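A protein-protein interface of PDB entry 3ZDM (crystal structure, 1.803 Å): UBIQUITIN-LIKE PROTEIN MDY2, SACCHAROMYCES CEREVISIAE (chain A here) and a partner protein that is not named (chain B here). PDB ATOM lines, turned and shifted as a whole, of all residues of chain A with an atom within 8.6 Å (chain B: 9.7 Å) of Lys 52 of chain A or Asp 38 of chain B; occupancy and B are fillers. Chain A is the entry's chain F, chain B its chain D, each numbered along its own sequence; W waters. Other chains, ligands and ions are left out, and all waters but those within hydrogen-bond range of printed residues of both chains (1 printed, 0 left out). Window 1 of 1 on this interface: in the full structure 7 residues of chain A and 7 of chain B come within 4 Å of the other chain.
The backbone NH of Thr 75 of chain A is in hydrogen-bond range of the backbone carbonyl oxygen of Leu 50 of chain A.
The backbone carbonyl oxygen (O) of Val 35 of chain B sits at hydrogen-bond distance from the side-chain sulfur (SG) of Cys 39 of chain B.
The side-chain carboxylate (OD1) of Asp 38 of chain B is in salt-bridge range of the guanidinium group (NH1) of Arg 48 of chain B, 3.0 Å away.
Among the printed residues, merely in contact across the chains: Leu 50 of chain A with Cys 39 of chain B (3.6 Å), Lys 52 of chain A with Asp 38 of chain B (3.8 Å), Gly 53 of chain A with Asp 38 of chain B (3.5 Å), Gly 53 of chain A with Cys 39 of chain B (3.6 Å), Gly 53 of chain A with Glu 42 of chain B (3.5 Å) and Lys 54 of chain A with Glu 42 of chain B (3.7 Å).
Of the printed residues of chain B, Leu 50 of chain A touches Cys 39.
Of the printed residues of chain B, Lys 54 of chain A touches Glu 42 (3.7 Å).
Asp 38 of chain B touches just these residues of chain A: Lys 52 and Gly 53.
Printed residues of chain A within 4 Å of Glu 42 of chain B: Gly 53 and Lys 54.
The nearest residue of chain B that does not touch Lys 52 of chain A is Cys 39 of chain B (4.7 Å).
The nearest printed residue of chain B that does not touch Leu 50 of chain A is Val 35 of chain B (5.0 Å).
Of the 14 printed residues of chain A, 4 touch a printed residue of chain B.
Of the 26 printed residues of chain B, 3 touch a printed residue of chain A.
Among the printed residues, 6 pairs touch across the chains.
Water W1 lies within hydrogen-bond range of the backbone NH of Gly 53 of chain A and the side-chain carboxylate of Glu 42 of chain B.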
ATOM      1  N   LEU A  49     -37.101  15.975 -27.888  1.00  0.00           N
ATOM      2  CA  LEU A  49     -36.214  17.118 -27.699  1.00  0.00           C
ATOM      3  C   LEU A  49     -35.984  17.260 -26.226  1.00  0.00           C
ATOM      4  O   LEU A  49     -36.913  17.048 -25.430  1.00  0.00           O
ATOM      5  CB  LEU A  49     -36.861  18.396 -28.217  1.00  0.00           C
ATOM      6  CG  LEU A  49     -37.189  18.422 -29.711  1.00  0.00           C
ATOM      7  CD1 LEU A  49     -37.747  19.804 -30.187  1.00  0.00           C
ATOM      8  CD2 LEU A  49     -35.965  18.035 -30.552  1.00  0.00           C
ATOM      9  N   LEU A  50     -34.744  17.593 -25.858  1.00  0.00           N
ATOM     10  CA  LEU A  50     -34.395  17.799 -24.491  1.00  0.00           C
ATOM     11  C   LEU A  50     -33.596  19.078 -24.325  1.00  0.00           C
ATOM     12  O   LEU A  50     -32.847  19.483 -25.230  1.00  0.00           O
ATOM     13  CB  LEU A  50     -33.523  16.652 -23.945  1.00  0.00           C
ATOM     14  CG  LEU A  50     -34.159  15.263 -23.954  1.00  0.00           C
ATOM     15  CD1 LEU A  50     -33.876  14.509 -25.240  1.00  0.00           C
ATOM     16  CD2 LEU A  50     -33.681  14.512 -22.761  1.00  0.00           C
ATOM     17  N   LEU A  51     -33.756  19.706 -23.159  1.00  0.00           N
ATOM     18  CA  LEU A  51     -32.829  20.747 -22.760  1.00  0.00           C
ATOM     19  C   LEU A  51     -32.165  20.216 -21.493  1.00  0.00           C
ATOM     20  O   LEU A  51     -32.836  20.028 -20.470  1.00  0.00           O
ATOM     21  CB  LEU A  51     -33.569  22.060 -22.500  1.00  0.00           C
ATOM     22  CG  LEU A  51     -32.619  23.193 -22.043  1.00  0.00           C
ATOM     23  CD1 LEU A  51     -31.490  23.473 -23.034  1.00  0.00           C
ATOM     24  CD2 LEU A  51     -33.394  24.448 -21.776  1.00  0.00           C
ATOM     25  N   LYS A  52     -30.867  19.955 -21.591  1.00  0.00           N
ATOM     26  CA  LYS A  52     -30.128  19.314 -20.529  1.00  0.00           C
ATOM     27  C   LYS A  52     -30.888  18.016 -20.262  1.00  0.00           C
ATOM     28  O   LYS A  52     -31.095  17.238 -21.183  1.00  0.00           O
ATOM     29  CB  LYS A  52     -30.095  20.205 -19.294  1.00  0.00           C
ATOM     30  CG  LYS A  52     -29.085  21.338 -19.297  1.00  0.00           C
ATOM     31  CD  LYS A  52     -28.680  21.667 -17.846  1.00  0.00           C
ATOM     32  CE  LYS A  52     -27.183  21.951 -17.732  1.00  0.00           C
ATOM     33  NZ  LYS A  52     -26.757  22.907 -18.795  1.00  0.00           N
ATOM     34  N   GLY A  53     -31.325  17.722 -19.047  1.00  0.00           N
ATOM     35  CA  GLY A  53     -31.965  16.400 -18.969  1.00  0.00           C
ATOM     36  C   GLY A  53     -33.493  16.355 -19.014  1.00  0.00           C
ATOM     37  O   GLY A  53     -34.146  15.311 -18.726  1.00  0.00           O
ATOM     38  N   LYS A  54     -34.077  17.485 -19.370  1.00  0.00           N
ATOM     39  CA  LYS A  54     -35.548  17.618 -19.380  1.00  0.00           C
ATOM     40  C   LYS A  54     -36.108  17.344 -20.797  1.00  0.00           C
ATOM     41  O   LYS A  54     -35.688  17.969 -21.769  1.00  0.00           O
ATOM     42  CB  LYS A  54     -35.917  19.010 -18.870  1.00  0.00           C
ATOM     43  CG  LYS A  54     -37.427  19.389 -18.858  1.00  0.00           C
ATOM     44  CD  LYS A  54     -37.557  20.881 -18.620  1.00  0.00           C
ATOM     45  CE  LYS A  54     -38.973  21.384 -18.831  1.00  0.00           C
ATOM     46  NZ  LYS A  54     -39.881  20.743 -17.860  1.00  0.00           N
ATOM     47  N   VAL A  55     -37.005  16.363 -20.895  1.00  0.00           N
ATOM     48  CA  VAL A  55     -37.715  16.060 -22.125  1.00  0.00           C
ATOM     49  C   VAL A  55     -38.813  17.098 -22.316  1.00  0.00           C
ATOM     50  O   VAL A  55     -39.622  17.305 -21.428  1.00  0.00           O
ATOM     51  CB  VAL A  55     -38.345  14.660 -22.090  1.00  0.00           C
ATOM     52  CG1 VAL A  55     -39.094  14.379 -23.393  1.00  0.00           C
ATOM     53  CG2 VAL A  55     -37.259  13.593 -21.901  1.00  0.00           C
ATOM     54  N   LEU A  56     -38.824  17.747 -23.478  1.00  0.00           N
ATOM     55  CA  LEU A  56     -39.675  18.917 -23.723  1.00  0.00           C
ATOM     56  C   LEU A  56     -40.979  18.540 -24.385  1.00  0.00           C
ATOM     57  O   LEU A  56     -40.990  17.924 -25.444  1.00  0.00           O
ATOM     58  CB  LEU A  56     -38.915  19.890 -24.632  1.00  0.00           C
ATOM     59  CG  LEU A  56     -37.532  20.282 -24.121  1.00  0.00           C
ATOM     60  CD1 LEU A  56     -36.826  21.230 -25.059  1.00  0.00           C
ATOM     61  CD2 LEU A  56     -37.619  20.914 -22.699  1.00  0.00           C
ATOM     62  N   VAL A  67     -33.866  29.854 -22.584  1.00  0.00           N
ATOM     63  CA  VAL A  67     -32.554  29.581 -23.162  1.00  0.00           C
ATOM     64  C   VAL A  67     -31.859  30.917 -23.400  1.00  0.00           C
ATOM     65  O   VAL A  67     -32.470  31.976 -23.270  1.00  0.00           O
ATOM     66  CB  VAL A  67     -32.638  28.781 -24.494  1.00  0.00           C
ATOM     67  CG1 VAL A  67     -33.192  27.371 -24.248  1.00  0.00           C
ATOM     68  CG2 VAL A  67     -33.462  29.507 -25.542  1.00  0.00           C
ATOM     69  N   SER A  72     -27.451  28.242 -26.762  1.00  0.00           N
ATOM     70  CA  SER A  72     -28.079  27.039 -26.215  1.00  0.00           C
ATOM     71  C   SER A  72     -28.286  25.950 -27.239  1.00  0.00           C
ATOM     72  O   SER A  72     -28.489  26.223 -28.442  1.00  0.00           O
ATOM     73  CB  SER A  72     -29.412  27.390 -25.541  1.00  0.00           C
ATOM     74  OG  SER A  72     -29.204  28.331 -24.491  1.00  0.00           O
ATOM     75  N   THR A  73     -28.294  24.711 -26.748  1.00  0.00           N
ATOM     76  CA  THR A  73     -28.414  23.550 -27.604  1.00  0.00           C
ATOM     77  C   THR A  73     -29.536  22.654 -27.141  1.00  0.00           C
ATOM     78  O   THR A  73     -29.639  22.326 -25.958  1.00  0.00           O
ATOM     79  CB  THR A  73     -27.098  22.718 -27.613  1.00  0.00           C
ATOM     80  OG1 THR A  73     -26.118  23.406 -28.387  1.00  0.00           O
ATOM     81  CG2 THR A  73     -27.326  21.390 -28.228  1.00  0.00           C
ATOM     82  N   ILE A  74     -30.378  22.266 -28.084  1.00  0.00           N
ATOM     83  CA  ILE A  74     -31.456  21.317 -27.836  1.00  0.00           C
ATOM     84  C   ILE A  74     -30.966  19.963 -28.301  1.00  0.00           C
ATOM     85  O   ILE A  74     -30.599  19.813 -29.460  1.00  0.00           O
ATOM     86  CB  ILE A  74     -32.752  21.656 -28.671  1.00  0.00           C
ATOM     87  CG1 ILE A  74     -33.243  23.073 -28.362  1.00  0.00           C
ATOM     88  CG2 ILE A  74     -33.830  20.610 -28.427  1.00  0.00           C
ATOM     89  CD1 ILE A  74     -33.371  23.331 -26.879  1.00  0.00           C
ATOM     90  N   THR A  75     -31.049  18.952 -27.434  1.00  0.00           N
ATOM     91  CA  THR A  75     -30.714  17.595 -27.833  1.00  0.00           C
ATOM     92  C   THR A  75     -31.849  16.929 -28.570  1.00  0.00           C
ATOM     93  O   THR A  75     -32.975  16.991 -28.100  1.00  0.00           O
ATOM     94  CB  THR A  75     -30.424  16.721 -26.591  1.00  0.00           C
ATOM     95  OG1 THR A  75     -29.422  17.370 -25.791  1.00  0.00           O
ATOM     96  CG2 THR A  75     -29.993  15.342 -26.948  1.00  0.00           C
ATOM     97  N   VAL A  76     -31.528  16.225 -29.655  1.00  0.00           N
ATOM     98  CA  VAL A  76     -32.516  15.599 -30.534  1.00  0.00           C
ATOM     99  C   VAL A  76     -32.323  14.100 -30.482  1.00  0.00           C
ATOM    100  O   VAL A  76     -31.217  13.611 -30.683  1.00  0.00           O
ATOM    101  CB  VAL A  76     -32.294  16.089 -31.971  1.00  0.00           C
ATOM    102  CG1 VAL A  76     -33.320  15.457 -32.925  1.00  0.00           C
ATOM    103  CG2 VAL A  76     -32.381  17.642 -32.011  1.00  0.00           C
ATOM    104  N   ALA B   9     -28.722   6.444  -7.988  1.00  0.00           N
ATOM    105  CA  ALA B   9     -28.603   7.271  -9.149  1.00  0.00           C
ATOM    106  C   ALA B   9     -27.350   8.113  -9.108  1.00  0.00           C
ATOM    107  O   ALA B   9     -26.703   8.303 -10.122  1.00  0.00           O
ATOM    108  CB  ALA B   9     -29.856   8.229  -9.287  1.00  0.00           C
ATOM    109  N   ILE B  12     -24.436   5.980 -10.035  1.00  0.00           N
ATOM    110  CA  ILE B  12     -24.425   5.697 -11.474  1.00  0.00           C
ATOM    111  C   ILE B  12     -23.871   6.910 -12.216  1.00  0.00           C
ATOM    112  O   ILE B  12     -23.016   6.791 -13.096  1.00  0.00           O
ATOM    113  CB  ILE B  12     -25.824   5.323 -11.974  1.00  0.00           C
ATOM    114  CG1 ILE B  12     -26.291   4.034 -11.271  1.00  0.00           C
ATOM    115  CG2 ILE B  12     -25.918   5.319 -13.539  1.00  0.00           C
ATOM    116  CD1 ILE B  12     -27.796   3.709 -11.559  1.00  0.00           C
ATOM    117  N   VAL B  13     -24.322   8.098 -11.829  1.00  0.00           N
ATOM    118  CA  VAL B  13     -23.793   9.317 -12.452  1.00  0.00           C
ATOM    119  C   VAL B  13     -22.275   9.420 -12.193  1.00  0.00           C
ATOM    120  O   VAL B  13     -21.491   9.778 -13.090  1.00  0.00           O
ATOM    121  CB  VAL B  13     -24.540  10.574 -11.964  1.00  0.00           C
ATOM    122  CG1 VAL B  13     -23.782  11.846 -12.387  1.00  0.00           C
ATOM    123  CG2 VAL B  13     -25.979  10.576 -12.567  1.00  0.00           C
ATOM    124  N   PHE B  16     -20.349   7.048 -14.575  1.00  0.00           N
ATOM    125  CA  PHE B  16     -20.237   7.578 -15.921  1.00  0.00           C
ATOM    126  C   PHE B  16     -19.320   8.782 -15.941  1.00  0.00           C
ATOM    127  O   PHE B  16     -18.607   9.038 -16.901  1.00  0.00           O
ATOM    128  CB  PHE B  16     -21.634   8.020 -16.408  1.00  0.00           C
ATOM    129  CG  PHE B  16     -22.603   6.862 -16.659  1.00  0.00           C
ATOM    130  CD1 PHE B  16     -22.127   5.570 -16.833  1.00  0.00           C
ATOM    131  CD2 PHE B  16     -23.976   7.098 -16.778  1.00  0.00           C
ATOM    132  CE1 PHE B  16     -23.009   4.493 -17.087  1.00  0.00           C
ATOM    133  CE2 PHE B  16     -24.877   6.048 -17.012  1.00  0.00           C
ATOM    134  CZ  PHE B  16     -24.410   4.754 -17.194  1.00  0.00           C
ATOM    135  N   SER B  17     -19.330   9.546 -14.861  1.00  0.00           N
ATOM    136  CA  SER B  17     -18.484  10.718 -14.813  1.00  0.00           C
ATOM    137  C   SER B  17     -17.006  10.306 -14.797  1.00  0.00           C
ATOM    138  O   SER B  17     -16.151  10.967 -15.397  1.00  0.00           O
ATOM    139  CB  SER B  17     -18.884  11.595 -13.609  1.00  0.00           C
ATOM    140  OG  SER B  17     -18.351  12.887 -13.754  1.00  0.00           O
ATOM    141  N   ALA B  30     -18.787   9.856 -25.023  1.00  0.00           N
ATOM    142  CA  ALA B  30     -18.787  10.796 -23.895  1.00  0.00           C
ATOM    143  C   ALA B  30     -19.997  11.747 -24.063  1.00  0.00           C
ATOM    144  O   ALA B  30     -20.655  12.065 -23.094  1.00  0.00           O
ATOM    145  CB  ALA B  30     -17.512  11.593 -23.860  1.00  0.00           C
ATOM    146  N   ASP B  31     -20.276  12.193 -25.292  1.00  0.00           N
ATOM    147  CA  ASP B  31     -21.469  13.027 -25.518  1.00  0.00           C
ATOM    148  C   ASP B  31     -22.752  12.297 -25.095  1.00  0.00           C
ATOM    149  O   ASP B  31     -23.648  12.899 -24.487  1.00  0.00           O
ATOM    150  CB  ASP B  31     -21.577  13.460 -26.986  1.00  0.00           C
ATOM    151  CG  ASP B  31     -20.553  14.550 -27.358  1.00  0.00           C
ATOM    152  OD1 ASP B  31     -19.923  15.187 -26.474  1.00  0.00           O
ATOM    153  OD2 ASP B  31     -20.375  14.771 -28.558  1.00  0.00           O
ATOM    154  N   SER B  32     -22.874  11.017 -25.463  1.00  0.00           N
ATOM    155  CA  SER B  32     -24.017  10.216 -25.013  1.00  0.00           C
ATOM    156  C   SER B  32     -24.117  10.087 -23.503  1.00  0.00           C
ATOM    157  O   SER B  32     -25.193  10.248 -22.948  1.00  0.00           O
ATOM    158  CB  SER B  32     -24.010   8.817 -25.646  1.00  0.00           C
ATOM    159  OG  SER B  32     -24.246   8.936 -27.055  1.00  0.00           O
ATOM    160  N   LEU B  33     -23.010   9.785 -22.821  1.00  0.00           N
ATOM    161  CA  LEU B  33     -23.091   9.694 -21.375  1.00  0.00           C
ATOM    162  C   LEU B  33     -23.421  11.045 -20.749  1.00  0.00           C
ATOM    163  O   LEU B  33     -24.023  11.079 -19.697  1.00  0.00           O
ATOM    164  CB  LEU B  33     -21.763   9.166 -20.807  1.00  0.00           C
ATOM    165  CG  LEU B  33     -21.510   7.703 -21.201  1.00  0.00           C
ATOM    166  CD1 LEU B  33     -20.166   7.207 -20.549  1.00  0.00           C
ATOM    167  CD2 LEU B  33     -22.730   6.837 -20.700  1.00  0.00           C
ATOM    168  N   ASN B  34     -22.940  12.149 -21.339  1.00  0.00           N
ATOM    169  CA  ASN B  34     -23.262  13.469 -20.795  1.00  0.00           C
ATOM    170  C   ASN B  34     -24.792  13.715 -20.823  1.00  0.00           C
ATOM    171  O   ASN B  34     -25.374  14.152 -19.829  1.00  0.00           O
ATOM    172  CB  ASN B  34     -22.521  14.561 -21.594  1.00  0.00           C
ATOM    173  CG  ASN B  34     -21.117  14.821 -21.068  1.00  0.00           C
ATOM    174  OD1 ASN B  34     -20.865  14.680 -19.877  1.00  0.00           O
ATOM    175  ND2 ASN B  34     -20.211  15.251 -21.943  1.00  0.00           N
ATOM    176  N   VAL B  35     -25.430  13.431 -21.947  1.00  0.00           N
ATOM    177  CA  VAL B  35     -26.903  13.448 -21.997  1.00  0.00           C
ATOM    178  C   VAL B  35     -27.525  12.511 -20.959  1.00  0.00           C
ATOM    179  O   VAL B  35     -28.440  12.904 -20.226  1.00  0.00           O
ATOM    180  CB  VAL B  35     -27.434  13.093 -23.395  1.00  0.00           C
ATOM    181  CG1 VAL B  35     -28.977  13.074 -23.407  1.00  0.00           C
ATOM    182  CG2 VAL B  35     -26.919  14.123 -24.397  1.00  0.00           C
ATOM    183  N   ALA B  36     -26.997  11.298 -20.855  1.00  0.00           N
ATOM    184  CA  ALA B  36     -27.512  10.333 -19.871  1.00  0.00           C
ATOM    185  C   ALA B  36     -27.365  10.891 -18.450  1.00  0.00           C
ATOM    186  O   ALA B  36     -28.278  10.763 -17.653  1.00  0.00           O
ATOM    187  CB  ALA B  36     -26.748   8.955 -19.982  1.00  0.00           C
ATOM    188  N   MET B  37     -26.209  11.488 -18.134  1.00  0.00           N
ATOM    189  CA  MET B  37     -25.997  12.016 -16.751  1.00  0.00           C
ATOM    190  C   MET B  37     -27.000  13.159 -16.462  1.00  0.00           C
ATOM    191  O   MET B  37     -27.563  13.235 -15.358  1.00  0.00           O
ATOM    192  CB  MET B  37     -24.564  12.426 -16.500  1.00  0.00           C
ATOM    193  CG  MET B  37     -23.626  11.217 -16.438  1.00  0.00           C
ATOM    194  SD  MET B  37     -21.954  11.738 -15.973  1.00  0.00           S
ATOM    195  CE  MET B  37     -21.266  12.103 -17.550  1.00  0.00           C
ATOM    196  N   ASP B  38     -27.199  14.048 -17.429  1.00  0.00           N
ATOM    197  CA  ASP B  38     -28.185  15.118 -17.227  1.00  0.00           C
ATOM    198  C   ASP B  38     -29.589  14.544 -17.016  1.00  0.00           C
ATOM    199  O   ASP B  38     -30.324  15.033 -16.149  1.00  0.00           O
ATOM    200  CB  ASP B  38     -28.202  16.080 -18.411  1.00  0.00           C
ATOM    201  CG  ASP B  38     -27.009  17.000 -18.418  1.00  0.00           C
ATOM    202  OD1 ASP B  38     -26.268  17.069 -17.386  1.00  0.00           O
ATOM    203  OD2 ASP B  38     -26.814  17.627 -19.465  1.00  0.00           O
ATOM    204  N   CYS B  39     -29.994  13.564 -17.839  1.00  0.00           N
ATOM    205  CA  CYS B  39     -31.306  12.908 -17.684  1.00  0.00           C
ATOM    206  C   CYS B  39     -31.481  12.232 -16.315  1.00  0.00           C
ATOM    207  O   CYS B  39     -32.536  12.323 -15.712  1.00  0.00           O
ATOM    208  CB  CYS B  39     -31.603  11.919 -18.810  1.00  0.00           C
ATOM    209  SG  CYS B  39     -31.735  12.605 -20.452  1.00  0.00           S
ATOM    210  N   ILE B  40     -30.462  11.563 -15.827  1.00  0.00           N
ATOM    211  CA  ILE B  40     -30.591  10.881 -14.556  1.00  0.00           C
ATOM    212  C   ILE B  40     -30.752  11.897 -13.433  1.00  0.00           C
ATOM    213  O   ILE B  40     -31.590  11.720 -12.534  1.00  0.00           O
ATOM    214  CB  ILE B  40     -29.365   9.983 -14.313  1.00  0.00           C
ATOM    215  CG1 ILE B  40     -29.341   8.875 -15.351  1.00  0.00           C
ATOM    216  CG2 ILE B  40     -29.414   9.424 -12.914  1.00  0.00           C
ATOM    217  CD1 ILE B  40     -27.950   8.134 -15.446  1.00  0.00           C
ATOM    218  N   SER B  41     -29.932  12.949 -13.498  1.00  0.00           N
ATOM    219  CA  SER B  41     -29.925  14.000 -12.494  1.00  0.00           C
ATOM    220  C   SER B  41     -31.283  14.688 -12.465  1.00  0.00           C
ATOM    221  O   SER B  41     -31.849  14.966 -11.406  1.00  0.00           O
ATOM    222  CB  SER B  41     -28.853  15.036 -12.828  1.00  0.00           C
ATOM    223  OG  SER B  41     -27.575  14.405 -12.718  1.00  0.00           O
ATOM    224  N   GLU B  42     -31.807  14.962 -13.657  1.00  0.00           N
ATOM    225  CA  GLU B  42     -33.126  15.556 -13.773  1.00  0.00           C
ATOM    226  C   GLU B  42     -34.181  14.638 -13.189  1.00  0.00           C
ATOM    227  O   GLU B  42     -35.023  15.085 -12.411  1.00  0.00           O
ATOM    228  CB  GLU B  42     -33.433  15.863 -15.221  1.00  0.00           C
ATOM    229  CG  GLU B  42     -34.902  16.347 -15.444  1.00  0.00           C
ATOM    230  CD  GLU B  42     -35.116  17.842 -15.265  1.00  0.00           C
ATOM    231  OE1 GLU B  42     -34.126  18.586 -15.191  1.00  0.00           O
ATOM    232  OE2 GLU B  42     -36.293  18.274 -15.262  1.00  0.00           O
ATOM    233  N   ALA B  43     -34.091  13.355 -13.517  1.00  0.00           N
ATOM    234  CA  ALA B  43     -35.087  12.391 -13.066  1.00  0.00           C
ATOM    235  C   ALA B  43     -35.113  12.239 -11.573  1.00  0.00           C
ATOM    236  O   ALA B  43     -36.167  12.076 -11.003  1.00  0.00           O
ATOM    237  CB  ALA B  43     -34.890  11.032 -13.719  1.00  0.00           C
ATOM    238  N   PHE B  44     -33.960  12.293 -10.930  1.00  0.00           N
ATOM    239  CA  PHE B  44     -33.903  12.036  -9.503  1.00  0.00           C
ATOM    240  C   PHE B  44     -33.846  13.292  -8.656  1.00  0.00           C
ATOM    241  O   PHE B  44     -33.809  13.217  -7.436  1.00  0.00           O
ATOM    242  CB  PHE B  44     -32.736  11.053  -9.178  1.00  0.00           C
ATOM    243  CG  PHE B  44     -33.029   9.627  -9.645  1.00  0.00           C
ATOM    244  CD1 PHE B  44     -33.737   8.758  -8.817  1.00  0.00           C
ATOM    245  CD2 PHE B  44     -32.692   9.205 -10.931  1.00  0.00           C
ATOM    246  CE1 PHE B  44     -34.050   7.470  -9.232  1.00  0.00           C
ATOM    247  CE2 PHE B  44     -32.997   7.901 -11.364  1.00  0.00           C
ATOM    248  CZ  PHE B  44     -33.675   7.031 -10.499  1.00  0.00           C
ATOM    249  N   GLY B  45     -33.837  14.448  -9.307  1.00  0.00           N
ATOM    250  CA  GLY B  45     -34.008  15.709  -8.602  1.00  0.00           C
ATOM    251  C   GLY B  45     -32.754  16.291  -7.984  1.00  0.00           C
ATOM    252  O   GLY B  45     -32.827  17.104  -7.063  1.00  0.00           O
ATOM    253  N   PHE B  46     -31.573  15.880  -8.443  1.00  0.00           N
ATOM    254  CA  PHE B  46     -30.371  16.552  -7.953  1.00  0.00           C
ATOM    255  C   PHE B  46     -29.598  17.214  -9.086  1.00  0.00           C
ATOM    256  O   PHE B  46     -29.823  16.887 -10.253  1.00  0.00           O
ATOM    257  CB  PHE B  46     -29.474  15.596  -7.128  1.00  0.00           C
ATOM    258  CG  PHE B  46     -29.073  14.324  -7.853  1.00  0.00           C
ATOM    259  CD1 PHE B  46     -28.105  14.345  -8.848  1.00  0.00           C
ATOM    260  CD2 PHE B  46     -29.681  13.109  -7.534  1.00  0.00           C
ATOM    261  CE1 PHE B  46     -27.719  13.175  -9.485  1.00  0.00           C
ATOM    262  CE2 PHE B  46     -29.313  11.930  -8.203  1.00  0.00           C
ATOM    263  CZ  PHE B  46     -28.343  11.968  -9.175  1.00  0.00           C
ATOM    264  N   GLU B  47     -28.720  18.161  -8.761  1.00  0.00           N
ATOM    265  CA  GLU B  47     -27.862  18.725  -9.784  1.00  0.00           C
ATOM    266  C   GLU B  47     -26.708  17.790  -9.965  1.00  0.00           C
ATOM    267  O   GLU B  47     -26.144  17.232  -9.027  1.00  0.00           O
ATOM    268  CB  GLU B  47     -27.275  20.078  -9.417  1.00  0.00           C
ATOM    269  CG  GLU B  47     -28.252  21.238  -9.320  1.00  0.00           C
ATOM    270  CD  GLU B  47     -28.932  21.480 -10.632  1.00  0.00           C
ATOM    271  OE1 GLU B  47     -28.247  21.870 -11.609  1.00  0.00           O
ATOM    272  OE2 GLU B  47     -30.148  21.236 -10.696  1.00  0.00           O
ATOM    273  N   ARG B  48     -26.355  17.606 -11.202  1.00  0.00           N
ATOM    274  CA  ARG B  48     -25.194  16.808 -11.529  1.00  0.00           C
ATOM    275  C   ARG B  48     -23.934  17.217 -10.729  1.00  0.00           C
ATOM    276  O   ARG B  48     -23.141  16.391 -10.266  1.00  0.00           O
ATOM    277  CB  ARG B  48     -25.001  16.991 -13.028  1.00  0.00           C
ATOM    278  CG  ARG B  48     -23.900  16.248 -13.585  1.00  0.00           C
ATOM    279  CD  ARG B  48     -24.005  16.347 -15.036  1.00  0.00           C
ATOM    280  NE  ARG B  48     -22.809  15.771 -15.603  1.00  0.00           N
ATOM    281  CZ  ARG B  48     -22.558  15.688 -16.895  1.00  0.00           C
ATOM    282  NH1 ARG B  48     -23.448  16.133 -17.797  1.00  0.00           N
ATOM    283  NH2 ARG B  48     -21.405  15.148 -17.277  1.00  0.00           N
ATOM    284  N   GLU B  49     -23.724  18.495 -10.518  1.00  0.00           N
ATOM    285  CA  GLU B  49     -22.591  18.997  -9.747  1.00  0.00           C
ATOM    286  C   GLU B  49     -22.704  18.710  -8.250  1.00  0.00           C
ATOM    287  O   GLU B  49     -21.763  18.938  -7.504  1.00  0.00           O
ATOM    288  CB  GLU B  49     -22.446  20.506  -9.958  1.00  0.00           C
ATOM    289  CG  GLU B  49     -22.125  20.899 -11.385  1.00  0.00           C
ATOM    290  CD  GLU B  49     -23.346  20.963 -12.323  1.00  0.00           C
ATOM    291  OE1 GLU B  49     -24.509  20.686 -11.906  1.00  0.00           O
ATOM    292  OE2 GLU B  49     -23.121  21.303 -13.509  1.00  0.00           O
ATOM    293  N   VAL B  51     -23.392  15.733  -7.041  1.00  0.00           N
ATOM    294  CA  VAL B  51     -23.127  14.322  -6.824  1.00  0.00           C
ATOM    295  C   VAL B  51     -21.927  14.056  -5.883  1.00  0.00           C
ATOM    296  O   VAL B  51     -22.020  13.234  -4.978  1.00  0.00           O
ATOM    297  CB  VAL B  51     -22.937  13.583  -8.172  1.00  0.00           C
ATOM    298  CG1 VAL B  51     -22.337  12.181  -7.917  1.00  0.00           C
ATOM    299  CG2 VAL B  51     -24.268  13.456  -8.877  1.00  0.00           C
HETATM  300  O   HOH W   1     -31.640  19.089 -16.746  1.00  0.00           O
